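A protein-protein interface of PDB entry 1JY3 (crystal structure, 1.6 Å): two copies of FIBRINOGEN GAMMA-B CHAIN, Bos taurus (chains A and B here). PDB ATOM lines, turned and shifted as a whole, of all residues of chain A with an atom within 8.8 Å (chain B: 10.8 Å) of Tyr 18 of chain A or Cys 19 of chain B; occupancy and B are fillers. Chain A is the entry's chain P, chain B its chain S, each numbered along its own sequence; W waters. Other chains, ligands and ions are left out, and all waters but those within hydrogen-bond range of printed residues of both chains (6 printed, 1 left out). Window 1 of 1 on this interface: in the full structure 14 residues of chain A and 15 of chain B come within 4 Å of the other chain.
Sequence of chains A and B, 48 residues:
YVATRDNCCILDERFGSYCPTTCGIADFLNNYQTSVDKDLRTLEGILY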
ATOM      1  N   ARG A   5       3.858 -27.336  11.832  1.00  0.00           N
ATOM      2  CA  ARG A   5       5.298 -27.175  12.048  1.00  0.00           C
ATOM      3  C   ARG A   5       6.170 -28.192  11.354  1.00  0.00           C
ATOM      4  O   ARG A   5       7.389 -28.078  11.425  1.00  0.00           O
ATOM      5  CB  ARG A   5       5.635 -27.099  13.539  1.00  0.00           C
ATOM      6  CG  ARG A   5       5.266 -25.755  14.135  1.00  0.00           C
ATOM      7  CD  ARG A   5       5.592 -25.620  15.631  1.00  0.00           C
ATOM      8  NE  ARG A   5       7.012 -25.352  15.863  1.00  0.00           N
ATOM      9  CZ  ARG A   5       7.912 -26.283  16.162  1.00  0.00           C
ATOM     10  NH1 ARG A   5       7.548 -27.566  16.277  1.00  0.00           N
ATOM     11  NH2 ARG A   5       9.172 -25.922  16.348  1.00  0.00           N
ATOM     12  N   ASP A   6       5.564 -29.179  10.690  1.00  0.00           N
ATOM     13  CA  ASP A   6       6.382 -30.113   9.916  1.00  0.00           C
ATOM     14  C   ASP A   6       6.274 -29.726   8.441  1.00  0.00           C
ATOM     15  O   ASP A   6       6.824 -30.414   7.579  1.00  0.00           O
ATOM     16  CB  ASP A   6       5.939 -31.567  10.099  1.00  0.00           C
ATOM     17  CG  ASP A   6       4.519 -31.821   9.652  1.00  0.00           C
ATOM     18  OD1 ASP A   6       4.128 -33.008   9.577  1.00  0.00           O
ATOM     19  OD2 ASP A   6       3.788 -30.850   9.371  1.00  0.00           O
ATOM     20  N   ASN A   7       5.609 -28.605   8.148  1.00  0.00           N
ATOM     21  CA  ASN A   7       5.412 -28.178   6.759  1.00  0.00           C
ATOM     22  C   ASN A   7       5.404 -26.648   6.639  1.00  0.00           C
ATOM     23  O   ASN A   7       4.663 -26.078   5.824  1.00  0.00           O
ATOM     24  CB  ASN A   7       4.076 -28.756   6.269  1.00  0.00           C
ATOM     25  CG  ASN A   7       3.919 -28.722   4.761  1.00  0.00           C
ATOM     26  OD1 ASN A   7       4.827 -29.087   4.022  1.00  0.00           O
ATOM     27  ND2 ASN A   7       2.724 -28.313   4.293  1.00  0.00           N
ATOM     28  N   CYS A   8       6.259 -25.980   7.412  1.00  0.00           N
ATOM     29  CA  CYS A   8       6.282 -24.513   7.392  1.00  0.00           C
ATOM     30  C   CYS A   8       7.639 -23.945   6.959  1.00  0.00           C
ATOM     31  O   CYS A   8       7.953 -22.761   7.175  1.00  0.00           O
ATOM     32  CB  CYS A   8       5.856 -23.982   8.781  1.00  0.00           C
ATOM     33  SG  CYS A   8       7.149 -24.143  10.049  1.00  0.00           S
ATOM     34  N   CYS A   9       8.434 -24.796   6.300  1.00  0.00           N
ATOM     35  CA  CYS A   9       9.756 -24.385   5.819  1.00  0.00           C
ATOM     36  C   CYS A   9      10.004 -24.936   4.422  1.00  0.00           C
ATOM     37  O   CYS A   9      11.081 -25.513   4.153  1.00  0.00           O
ATOM     38  CB  CYS A   9      10.835 -24.922   6.771  1.00  0.00           C
ATOM     39  SG  CYS A   9      12.513 -24.269   6.514  1.00  0.00           S
ATOM     40  N   ILE A  10       9.032 -24.746   3.525  1.00  0.00           N
ATOM     41  CA  ILE A  10       9.162 -25.270   2.160  1.00  0.00           C
ATOM     42  C   ILE A  10      10.051 -24.336   1.352  1.00  0.00           C
ATOM     43  O   ILE A  10       9.616 -23.248   0.942  1.00  0.00           O
ATOM     44  CB  ILE A  10       7.774 -25.397   1.481  1.00  0.00           C
ATOM     45  CG1 ILE A  10       6.896 -26.379   2.261  1.00  0.00           C
ATOM     46  CG2 ILE A  10       7.958 -25.887   0.034  1.00  0.00           C
ATOM     47  CD1 ILE A  10       5.429 -26.433   1.765  1.00  0.00           C
ATOM     48  N   LEU A  11      11.286 -24.760   1.085  1.00  0.00           N
ATOM     49  CA  LEU A  11      12.230 -23.913   0.363  1.00  0.00           C
ATOM     50  C   LEU A  11      12.415 -24.293  -1.123  1.00  0.00           C
ATOM     51  O   LEU A  11      13.137 -23.613  -1.872  1.00  0.00           O
ATOM     52  CB  LEU A  11      13.580 -23.892   1.123  1.00  0.00           C
ATOM     53  CG  LEU A  11      13.498 -23.508   2.609  1.00  0.00           C
ATOM     54  CD1 LEU A  11      14.896 -23.456   3.248  1.00  0.00           C
ATOM     55  CD2 LEU A  11      12.841 -22.141   2.724  1.00  0.00           C
ATOM     56  N   ASP A  12      11.783 -25.387  -1.519  1.00  0.00           N
ATOM     57  CA  ASP A  12      11.787 -25.862  -2.903  1.00  0.00           C
ATOM     58  C   ASP A  12      10.469 -26.613  -3.030  1.00  0.00           C
ATOM     59  O   ASP A  12      10.235 -27.613  -2.338  1.00  0.00           O
ATOM     60  CB  ASP A  12      12.966 -26.804  -3.174  1.00  0.00           C
ATOM     61  CG  ASP A  12      13.065 -27.198  -4.638  1.00  0.00           C
ATOM     62  OD1 ASP A  12      12.055 -27.647  -5.232  1.00  0.00           O
ATOM     63  OD2 ASP A  12      14.163 -27.058  -5.201  1.00  0.00           O
ATOM     64  N   GLU A  13       9.589 -26.125  -3.904  1.00  0.00           N
ATOM     65  CA  GLU A  13       8.284 -26.733  -4.053  1.00  0.00           C
ATOM     66  C   GLU A  13       8.278 -28.203  -4.448  1.00  0.00           C
ATOM     67  O   GLU A  13       7.312 -28.909  -4.153  1.00  0.00           O
ATOM     68  CB  GLU A  13       7.433 -25.914  -5.046  1.00  0.00           C
ATOM     69  CG  GLU A  13       8.008 -25.824  -6.447  1.00  0.00           C
ATOM     70  CD  GLU A  13       7.150 -24.985  -7.379  1.00  0.00           C
ATOM     71  OE1 GLU A  13       6.934 -23.790  -7.075  1.00  0.00           O
ATOM     72  OE2 GLU A  13       6.694 -25.515  -8.414  1.00  0.00           O
ATOM     73  N   ARG A  14       9.365 -28.684  -5.059  1.00  0.00           N
ATOM     74  CA  ARG A  14       9.395 -30.089  -5.469  1.00  0.00           C
ATOM     75  C   ARG A  14      10.027 -31.019  -4.417  1.00  0.00           C
ATOM     76  O   ARG A  14       9.880 -32.233  -4.501  1.00  0.00           O
ATOM     77  CB  ARG A  14      10.159 -30.267  -6.807  1.00  0.00           C
ATOM     78  CG  ARG A  14       9.591 -29.411  -7.952  1.00  0.00           C
ATOM     79  CD  ARG A  14      10.060 -29.948  -9.289  1.00  0.00           C
ATOM     80  NE  ARG A  14      11.513 -29.971  -9.370  1.00  0.00           N
ATOM     81  CZ  ARG A  14      12.188 -30.720 -10.240  1.00  0.00           C
ATOM     82  NH1 ARG A  14      11.520 -31.500 -11.090  1.00  0.00           N
ATOM     83  NH2 ARG A  14      13.511 -30.687 -10.242  1.00  0.00           N
ATOM     84  N   PHE A  15      10.695 -30.447  -3.420  1.00  0.00           N
ATOM     85  CA  PHE A  15      11.339 -31.247  -2.383  1.00  0.00           C
ATOM     86  C   PHE A  15      10.751 -31.098  -0.981  1.00  0.00           C
ATOM     87  O   PHE A  15      11.185 -31.758  -0.053  1.00  0.00           O
ATOM     88  CB  PHE A  15      12.835 -30.956  -2.358  1.00  0.00           C
ATOM     89  CG  PHE A  15      13.584 -31.599  -3.491  1.00  0.00           C
ATOM     90  CD1 PHE A  15      13.822 -30.910  -4.681  1.00  0.00           C
ATOM     91  CD2 PHE A  15      14.031 -32.908  -3.373  1.00  0.00           C
ATOM     92  CE1 PHE A  15      14.517 -31.540  -5.761  1.00  0.00           C
ATOM     93  CE2 PHE A  15      14.719 -33.556  -4.421  1.00  0.00           C
ATOM     94  CZ  PHE A  15      14.964 -32.870  -5.619  1.00  0.00           C
ATOM     95  N   GLY A  16       9.751 -30.243  -0.841  1.00  0.00           N
ATOM     96  CA  GLY A  16       9.099 -30.126   0.456  1.00  0.00           C
ATOM     97  C   GLY A  16       9.678 -29.234   1.535  1.00  0.00           C
ATOM     98  O   GLY A  16      10.468 -28.333   1.261  1.00  0.00           O
ATOM     99  N   SER A  17       9.299 -29.520   2.779  1.00  0.00           N
ATOM    100  CA  SER A  17       9.717 -28.699   3.918  1.00  0.00           C
ATOM    101  C   SER A  17      11.065 -29.167   4.493  1.00  0.00           C
ATOM    102  O   SER A  17      11.306 -30.377   4.670  1.00  0.00           O
ATOM    103  CB  SER A  17       8.590 -28.699   4.975  1.00  0.00           C
ATOM    104  OG  SER A  17       8.760 -27.606   5.857  1.00  0.00           O
ATOM    105  N   TYR A  18      11.904 -28.187   4.801  1.00  0.00           N
ATOM    106  CA  TYR A  18      13.291 -28.423   5.235  1.00  0.00           C
ATOM    107  C   TYR A  18      13.510 -28.523   6.726  1.00  0.00           C
ATOM    108  O   TYR A  18      12.739 -27.999   7.541  1.00  0.00           O
ATOM    109  CB  TYR A  18      14.169 -27.309   4.655  1.00  0.00           C
ATOM    110  CG  TYR A  18      14.478 -27.374   3.149  1.00  0.00           C
ATOM    111  CD1 TYR A  18      13.541 -27.851   2.217  1.00  0.00           C
ATOM    112  CD2 TYR A  18      15.711 -26.920   2.671  1.00  0.00           C
ATOM    113  CE1 TYR A  18      13.833 -27.870   0.837  1.00  0.00           C
ATOM    114  CE2 TYR A  18      16.001 -26.925   1.293  1.00  0.00           C
ATOM    115  CZ  TYR A  18      15.073 -27.395   0.397  1.00  0.00           C
ATOM    116  OH  TYR A  18      15.422 -27.365  -0.952  1.00  0.00           O
ATOM    117  N   CYS A  19      14.579 -29.241   7.085  1.00  0.00           N
ATOM    118  CA  CYS A  19      15.003 -29.457   8.475  1.00  0.00           C
ATOM    119  C   CYS A  19      16.509 -29.460   8.578  1.00  0.00           C
ATOM    120  O   CYS A  19      17.210 -29.663   7.571  1.00  0.00           O
ATOM    121  CB  CYS A  19      14.599 -30.849   8.989  1.00  0.00           C
ATOM    122  SG  CYS A  19      12.805 -31.078   9.067  1.00  0.00           S
ATOM    123  N   PRO A  20      17.041 -29.219   9.774  1.00  0.00           N
ATOM    124  CA  PRO A  20      18.510 -29.267   9.885  1.00  0.00           C
ATOM    125  C   PRO A  20      18.935 -30.722   9.669  1.00  0.00           C
ATOM    126  O   PRO A  20      18.108 -31.639   9.730  1.00  0.00           O
ATOM    127  CB  PRO A  20      18.790 -28.813  11.322  1.00  0.00           C
ATOM    128  CG  PRO A  20      17.505 -29.194  12.044  1.00  0.00           C
ATOM    129  CD  PRO A  20      16.414 -28.835  11.058  1.00  0.00           C
ATOM    130  N   THR A  21      20.226 -30.938   9.409  1.00  0.00           N
ATOM    131  CA  THR A  21      20.709 -32.315   9.223  1.00  0.00           C
ATOM    132  C   THR A  21      21.065 -32.893  10.589  1.00  0.00           C
ATOM    133  O   THR A  21      21.195 -32.145  11.578  1.00  0.00           O
ATOM    134  CB  THR A  21      22.010 -32.375   8.357  1.00  0.00           C
ATOM    135  OG1 THR A  21      23.105 -31.819   9.096  1.00  0.00           O
ATOM    136  CG2 THR A  21      21.841 -31.620   7.040  1.00  0.00           C
ATOM    137  N   THR A  22      21.269 -34.206  10.649  1.00  0.00           N
ATOM    138  CA  THR A  22      21.665 -34.801  11.925  1.00  0.00           C
ATOM    139  C   THR A  22      23.134 -34.450  12.228  1.00  0.00           C
ATOM    140  O   THR A  22      23.589 -34.666  13.360  1.00  0.00           O
ATOM    141  CB  THR A  22      21.464 -36.306  11.928  1.00  0.00           C
ATOM    142  OG1 THR A  22      21.983 -36.836  10.701  1.00  0.00           O
ATOM    143  CG2 THR A  22      19.951 -36.636  12.076  1.00  0.00           C
ATOM    144  N   VAL B   2      17.681 -19.034   0.909  1.00  0.00           N
ATOM    145  CA  VAL B   2      18.228 -19.401   2.250  1.00  0.00           C
ATOM    146  C   VAL B   2      17.040 -19.434   3.223  1.00  0.00           C
ATOM    147  O   VAL B   2      16.074 -18.708   3.013  1.00  0.00           O
ATOM    148  CB  VAL B   2      19.237 -18.332   2.763  1.00  0.00           C
ATOM    149  CG1 VAL B   2      20.167 -18.952   3.787  1.00  0.00           C
ATOM    150  CG2 VAL B   2      20.020 -17.755   1.607  1.00  0.00           C
ATOM    151  N   ALA B   3      17.109 -20.269   4.258  1.00  0.00           N
ATOM    152  CA  ALA B   3      16.035 -20.342   5.253  1.00  0.00           C
ATOM    153  C   ALA B   3      16.097 -19.046   6.080  1.00  0.00           C
ATOM    154  O   ALA B   3      17.187 -18.611   6.462  1.00  0.00           O
ATOM    155  CB  ALA B   3      16.233 -21.558   6.165  1.00  0.00           C
ATOM    156  N   THR B   4      14.941 -18.434   6.329  1.00  0.00           N
ATOM    157  CA  THR B   4      14.878 -17.211   7.135  1.00  0.00           C
ATOM    158  C   THR B   4      13.702 -17.361   8.089  1.00  0.00           C
ATOM    159  O   THR B   4      12.890 -18.262   7.961  1.00  0.00           O
ATOM    160  CB  THR B   4      14.586 -15.950   6.294  1.00  0.00           C
ATOM    161  OG1 THR B   4      13.265 -16.047   5.733  1.00  0.00           O
ATOM    162  CG2 THR B   4      15.590 -15.817   5.182  1.00  0.00           C
ATOM    163  N   ASN B   7      10.427 -17.394   6.010  1.00  0.00           N
ATOM    164  CA  ASN B   7       9.996 -18.475   5.132  1.00  0.00           C
ATOM    165  C   ASN B   7      10.188 -19.845   5.772  1.00  0.00           C
ATOM    166  O   ASN B   7       9.912 -20.866   5.133  1.00  0.00           O
ATOM    167  CB  ASN B   7      10.766 -18.427   3.783  1.00  0.00           C
ATOM    168  CG  ASN B   7      12.257 -18.704   3.938  1.00  0.00           C
ATOM    169  OD1 ASN B   7      12.691 -19.317   4.906  1.00  0.00           O
ATOM    170  ND2 ASN B   7      13.043 -18.264   2.968  1.00  0.00           N
ATOM    171  N   CYS B   8      10.584 -19.865   7.042  1.00  0.00           N
ATOM    172  CA  CYS B   8      10.866 -21.126   7.726  1.00  0.00           C
ATOM    173  C   CYS B   8      10.485 -20.933   9.189  1.00  0.00           C
ATOM    174  O   CYS B   8      11.317 -20.498  10.001  1.00  0.00           O
ATOM    175  CB  CYS B   8      12.353 -21.401   7.555  1.00  0.00           C
ATOM    176  SG  CYS B   8      12.875 -23.055   8.111  1.00  0.00           S
ATOM    177  N   CYS B   9       9.245 -21.308   9.520  1.00  0.00           N
ATOM    178  CA  CYS B   9       8.722 -21.045  10.857  1.00  0.00           C
ATOM    179  C   CYS B   9       9.373 -21.728  12.039  1.00  0.00           C
ATOM    180  O   CYS B   9       9.168 -21.301  13.190  1.00  0.00           O
ATOM    181  CB  CYS B   9       7.190 -21.237  10.878  1.00  0.00           C
ATOM    182  SG  CYS B   9       6.543 -22.826  11.474  1.00  0.00           S
ATOM    183  N   ILE B  10      10.181 -22.750  11.786  1.00  0.00           N
ATOM    184  CA  ILE B  10      10.850 -23.452  12.879  1.00  0.00           C
ATOM    185  C   ILE B  10      12.341 -23.124  12.941  1.00  0.00           C
ATOM    186  O   ILE B  10      13.049 -23.636  13.792  1.00  0.00           O
ATOM    187  CB  ILE B  10      10.692 -25.031  12.777  1.00  0.00           C
ATOM    188  CG1 ILE B  10      11.476 -25.612  11.581  1.00  0.00           C
ATOM    189  CG2 ILE B  10       9.204 -25.425  12.735  1.00  0.00           C
ATOM    190  CD1 ILE B  10      11.315 -24.924  10.306  1.00  0.00           C
ATOM    191  N   LEU B  11      12.812 -22.226  12.072  1.00  0.00           N
ATOM    192  CA  LEU B  11      14.245 -21.936  11.996  1.00  0.00           C
ATOM    193  C   LEU B  11      14.969 -21.572  13.294  1.00  0.00           C
ATOM    194  O   LEU B  11      14.538 -20.690  14.045  1.00  0.00           O
ATOM    195  CB  LEU B  11      14.522 -20.827  10.954  1.00  0.00           C
ATOM    196  CG  LEU B  11      16.008 -20.388  10.844  1.00  0.00           C
ATOM    197  CD1 LEU B  11      16.885 -21.511  10.281  1.00  0.00           C
ATOM    198  CD2 LEU B  11      16.127 -19.131   9.929  1.00  0.00           C
ATOM    199  N   ASP B  12      16.044 -22.309  13.567  1.00  0.00           N
ATOM    200  CA  ASP B  12      16.961 -22.023  14.683  1.00  0.00           C
ATOM    201  C   ASP B  12      18.312 -22.325  14.041  1.00  0.00           C
ATOM    202  O   ASP B  12      18.744 -23.477  13.964  1.00  0.00           O
ATOM    203  CB  ASP B  12      16.706 -22.913  15.925  1.00  0.00           C
ATOM    204  CG  ASP B  12      17.569 -22.500  17.111  1.00  0.00           C
ATOM    205  OD1 ASP B  12      17.141 -22.713  18.275  1.00  0.00           O
ATOM    206  OD2 ASP B  12      18.709 -21.976  16.899  1.00  0.00           O
ATOM    207  N   PHE B  15      21.427 -24.795  14.734  1.00  0.00           N
ATOM    208  CA  PHE B  15      21.417 -26.181  14.285  1.00  0.00           C
ATOM    209  C   PHE B  15      21.934 -26.392  12.867  1.00  0.00           C
ATOM    210  O   PHE B  15      21.826 -27.480  12.340  1.00  0.00           O
ATOM    211  CB  PHE B  15      20.011 -26.778  14.476  1.00  0.00           C
ATOM    212  CG  PHE B  15      19.624 -26.914  15.921  1.00  0.00           C
ATOM    213  CD1 PHE B  15      19.090 -25.816  16.622  1.00  0.00           C
ATOM    214  CD2 PHE B  15      19.875 -28.096  16.600  1.00  0.00           C
ATOM    215  CE1 PHE B  15      18.816 -25.906  18.009  1.00  0.00           C
ATOM    216  CE2 PHE B  15      19.608 -28.213  17.976  1.00  0.00           C
ATOM    217  CZ  PHE B  15      19.079 -27.113  18.681  1.00  0.00           C
ATOM    218  N   GLY B  16      22.467 -25.330  12.277  1.00  0.00           N
ATOM    219  CA  GLY B  16      23.073 -25.410  10.953  1.00  0.00           C
ATOM    220  C   GLY B  16      22.185 -25.165   9.764  1.00  0.00           C
ATOM    221  O   GLY B  16      21.019 -24.806   9.897  1.00  0.00           O
ATOM    222  N   SER B  17      22.745 -25.348   8.571  1.00  0.00           N
ATOM    223  CA  SER B  17      21.970 -25.165   7.352  1.00  0.00           C
ATOM    224  C   SER B  17      20.841 -26.192   7.237  1.00  0.00           C
ATOM    225  O   SER B  17      20.935 -27.284   7.789  1.00  0.00           O
ATOM    226  CB  SER B  17      22.900 -25.278   6.132  1.00  0.00           C
ATOM    227  OG  SER B  17      23.356 -26.624   6.022  1.00  0.00           O
ATOM    228  N   TYR B  18      19.754 -25.841   6.563  1.00  0.00           N
ATOM    229  CA  TYR B  18      18.640 -26.775   6.426  1.00  0.00           C
ATOM    230  C   TYR B  18      18.597 -27.417   5.051  1.00  0.00           C
ATOM    231  O   TYR B  18      19.058 -26.831   4.047  1.00  0.00           O
ATOM    232  CB  TYR B  18      17.309 -26.059   6.727  1.00  0.00           C
ATOM    233  CG  TYR B  18      16.988 -25.815   8.202  1.00  0.00           C
ATOM    234  CD1 TYR B  18      17.982 -25.700   9.173  1.00  0.00           C
ATOM    235  CD2 TYR B  18      15.658 -25.630   8.603  1.00  0.00           C
ATOM    236  CE1 TYR B  18      17.656 -25.403  10.543  1.00  0.00           C
ATOM    237  CE2 TYR B  18      15.337 -25.328   9.944  1.00  0.00           C
ATOM    238  CZ  TYR B  18      16.335 -25.221  10.883  1.00  0.00           C
ATOM    239  OH  TYR B  18      15.991 -24.936  12.191  1.00  0.00           O
ATOM    240  N   CYS B  19      18.021 -28.628   5.019  1.00  0.00           N
ATOM    241  CA  CYS B  19      17.932 -29.472   3.806  1.00  0.00           C
ATOM    242  C   CYS B  19      16.585 -30.173   3.725  1.00  0.00           C
ATOM    243  O   CYS B  19      15.863 -30.246   4.719  1.00  0.00           O
ATOM    244  CB  CYS B  19      18.932 -30.643   3.930  1.00  0.00           C
ATOM    245  SG  CYS B  19      20.660 -30.125   3.943  1.00  0.00           S
ATOM    246  N   PRO B  20      16.233 -30.725   2.549  1.00  0.00           N
ATOM    247  CA  PRO B  20      14.968 -31.464   2.445  1.00  0.00           C
ATOM    248  C   PRO B  20      15.120 -32.651   3.457  1.00  0.00           C
ATOM    249  O   PRO B  20      16.228 -33.010   3.867  1.00  0.00           O
ATOM    250  CB  PRO B  20      15.016 -32.024   1.013  1.00  0.00           C
ATOM    251  CG  PRO B  20      15.764 -30.940   0.250  1.00  0.00           C
ATOM    252  CD  PRO B  20      16.862 -30.527   1.220  1.00  0.00           C
ATOM    253  N   THR B  21      14.011 -33.245   3.868  1.00  0.00           N
ATOM    254  CA  THR B  21      14.101 -34.448   4.692  1.00  0.00           C
ATOM    255  C   THR B  21      14.119 -35.610   3.693  1.00  0.00           C
ATOM    256  O   THR B  21      13.842 -35.428   2.500  1.00  0.00           O
ATOM    257  CB  THR B  21      12.853 -34.634   5.577  1.00  0.00           C
ATOM    258  OG1 THR B  21      11.677 -34.781   4.745  1.00  0.00           O
ATOM    259  CG2 THR B  21      12.682 -33.442   6.472  1.00  0.00           C
ATOM    260  N   THR B  22      14.431 -36.817   4.165  1.00  0.00           N
ATOM    261  CA  THR B  22      14.371 -37.962   3.271  1.00  0.00           C
ATOM    262  C   THR B  22      12.929 -38.318   2.900  1.00  0.00           C
ATOM    263  O   THR B  22      12.701 -39.101   1.971  1.00  0.00           O
ATOM    264  CB  THR B  22      15.053 -39.192   3.852  1.00  0.00           C
ATOM    265  OG1 THR B  22      14.585 -39.408   5.186  1.00  0.00           O
ATOM    266  CG2 THR B  22      16.562 -38.995   3.849  1.00  0.00           C
ATOM    267  N   CYS B  23      11.944 -37.780   3.630  1.00  0.00           N
ATOM    268  CA  CYS B  23      10.542 -37.979   3.209  1.00  0.00           C
ATOM    269  C   CYS B  23      10.341 -37.141   1.928  1.00  0.00           C
ATOM    270  O   CYS B  23       9.725 -37.607   0.977  1.00  0.00           O
ATOM    271  CB  CYS B  23       9.533 -37.502   4.262  1.00  0.00           C
ATOM    272  SG  CYS B  23       9.376 -38.538   5.740  1.00  0.00           S
ATOM    273  N   GLY B  24      10.855 -35.910   1.909  1.00  0.00           N
ATOM    274  CA  GLY B  24      10.751 -35.077   0.724  1.00  0.00           C
ATOM    275  C   GLY B  24      11.487 -35.747  -0.433  1.00  0.00           C
ATOM    276  O   GLY B  24      11.030 -35.714  -1.569  1.00  0.00           O
ATOM    277  N   ILE B  25      12.627 -36.372  -0.142  1.00  0.00           N
ATOM    278  CA  ILE B  25      13.388 -37.061  -1.197  1.00  0.00           C
ATOM    279  C   ILE B  25      12.560 -38.231  -1.762  1.00  0.00           C
ATOM    280  O   ILE B  25      12.491 -38.409  -2.969  1.00  0.00           O
ATOM    281  CB  ILE B  25      14.728 -37.610  -0.624  1.00  0.00           C
ATOM    282  CG1 ILE B  25      15.654 -36.447  -0.214  1.00  0.00           C
ATOM    283  CG2 ILE B  25      15.441 -38.502  -1.671  1.00  0.00           C
ATOM    284  CD1 ILE B  25      15.916 -35.416  -1.311  1.00  0.00           C
ATOM    285  N   PHE B  28       9.696 -36.872  -3.913  1.00  0.00           N
ATOM    286  CA  PHE B  28      10.213 -36.369  -5.187  1.00  0.00           C
ATOM    287  C   PHE B  28      10.517 -37.584  -6.078  1.00  0.00           C
ATOM    288  O   PHE B  28      10.151 -37.598  -7.255  1.00  0.00           O
ATOM    289  CB  PHE B  28      11.504 -35.557  -4.989  1.00  0.00           C
ATOM    290  CG  PHE B  28      12.135 -35.078  -6.286  1.00  0.00           C
ATOM    291  CD1 PHE B  28      11.932 -33.787  -6.730  1.00  0.00           C
ATOM    292  CD2 PHE B  28      12.884 -35.940  -7.078  1.00  0.00           C
ATOM    293  CE1 PHE B  28      12.457 -33.357  -7.947  1.00  0.00           C
ATOM    294  CE2 PHE B  28      13.414 -35.526  -8.303  1.00  0.00           C
ATOM    295  CZ  PHE B  28      13.203 -34.236  -8.740  1.00  0.00           C
HETATM  296  O   HOH W   1       9.467 -33.065   5.456  1.00  0.00           O
HETATM  297  O   HOH W   2      11.471 -23.432  16.316  1.00  0.00           O
HETATM  298  O   HOH W   3       7.643 -22.595  15.513  1.00  0.00           O
HETATM  299  O   HOH W   4       8.613 -21.099   2.808  1.00  0.00           O
HETATM  300  O   HOH W   5      11.612 -32.222   2.582  1.00  0.00           O
HETATM  301  O   HOH W   6      22.128 -28.616   9.840  1.00  0.00           O
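The side-chain sulfur (SG) of Cys 8 of chain A is disulfide-bonded to the side-chain sulfur (SG) of Cys 9 of chain B (2.0 Å). The side-chain sulfur (SG) of Cys 8 of chain A sits close to the backbone NH (N) of Ile 10 of chain B (3.8 Å). The side-chain sulfur (SG) of Cys 9 of chain A is disulfide-bonded to the side-chain sulfur (SG) of Cys 8 of chain B, 2.0 Å away. The backbone carbonyl oxygen of Cys 19 of chain A sits at hydrogen-bond distance from the backbone NH of Cys 19 of chain B, 2.9 Å away. The backbone carbonyl oxygen of Asn 7 of chain B lies close to the backbone carbonyl oxygen of Cys 8 of chain A, at 3.4 Å.
OD1 of Asp 12 of chain A is in hydrogen-bond range of N of Arg 14 of chain A (2.9 Å). The backbone carbonyl oxygen (O) of Val 2 of chain B is in hydrogen-bond range of the side-chain amide nitrogen (ND2) of Asn 7 of chain B (3.1 Å). OG1 of Thr 21 of chain B lies within hydrogen-bond range of N of Gly 24 of chain B.
Among the printed residues, pairs that only touch across the chains: Tyr 18 of chain A with Cys 19 of chain B (3.2 Å), Phe 15 of chain A with Phe 28 of chain B (3.4 Å), Cys 8 of chain A with Cys 8 of chain B (3.4 Å), Arg 14 of chain A with Phe 28 of chain B (3.4 Å), Cys 19 of chain A with Tyr 18 of chain B (3.4 Å), Phe 15 of chain A with Gly 24 of chain B (3.4 Å), Pro 20 of chain A with Phe 15 of chain B (3.5 Å), Arg 5 of chain A with Ile 10 of chain B (3.5 Å), Cys 19 of chain A with Thr 21 of chain B (3.5 Å), Cys 9 of chain A with Ile 10 of chain B (3.6 Å), Leu 11 of chain A with Asn 7 of chain B (3.6 Å), Cys 9 of chain A with Asn 7 of chain B (3.6 Å), Tyr 18 of chain A with Pro 20 of chain B (3.6 Å), Pro 20 of chain A with Tyr 18 of chain B (3.6 Å), Tyr 18 of chain A with Tyr 18 of chain B (3.6 Å), Thr 21 of chain A with Cys 19 of chain B (3.6 Å), Leu 11 of chain A with Ala 3 of chain B (3.7 Å), Phe 15 of chain A with Ile 25 of chain B (3.8 Å), Pro 20 of chain A with Ser 17 of chain B (3.8 Å), Ser 17 of chain A with Thr 21 of chain B (3.8 Å) and Phe 15 of chain A with Pro 20 of chain B (3.9 Å).
Of the printed residues of chain B, Cys 9 of chain A touches Asn 7, Cys 8 and Ile 10. Leu 11 of chain A touches just these residues of chain B: Ala 3 (3.7 Å) and Asn 7 (3.6 Å). Glu 13 of chain A touches none of the printed residues of chain B. Of chain B, only Thr 21 (3.8 Å) comes within 4 Å of Ser 17 of chain A. Of chain B, only Phe 15 (3.5 Å), Ser 17 (3.8 Å) and Tyr 18 (3.6 Å) come within 4 Å of Pro 20 of chain A. Of the printed residues of chain A, Gly 24 of chain B touches Phe 15.
Printed residues of chain A that touch a printed residue of chain B: Arg 5, Cys 8, Cys 9, Leu 11, Arg 14, Phe 15, Ser 17, Tyr 18, Cys 19, Pro 20 and Thr 21. Hydrophobic or aromatic side chains of chain A that line the printed part of chain B: Leu 11, Phe 15, Tyr 18 and Pro 20. Hydrophobic or aromatic side chains of chain B that line the printed part of chain A: Ala 3, Ile 10, Phe 15, Tyr 18, Pro 20, Ile 25 and Phe 28. Among the printed residues, 26 pairs touch across the chains.
Cys 8 of chain A touches Asn 7 of chain B, but with the chains exchanged Asn 7 of chain A does not touch Cys 8 of chain B (7.8 Å). Positions printed for both chains: 7, 8, 9, 10, 11, 12, 15, 16, 17, 18, 19, 20, 21 and 22.
Water W6 lies within hydrogen-bond range of O of Ser 17 of chain B (2.7 Å), O of Phe 15 of chain B (2.8 Å) and N of Thr 21 of chain A (3.0 Å). Water W2 bridges O of Ile 10 of chain B (3.0 Å) and NH2 of Arg 5 of chain A (3.4 Å).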
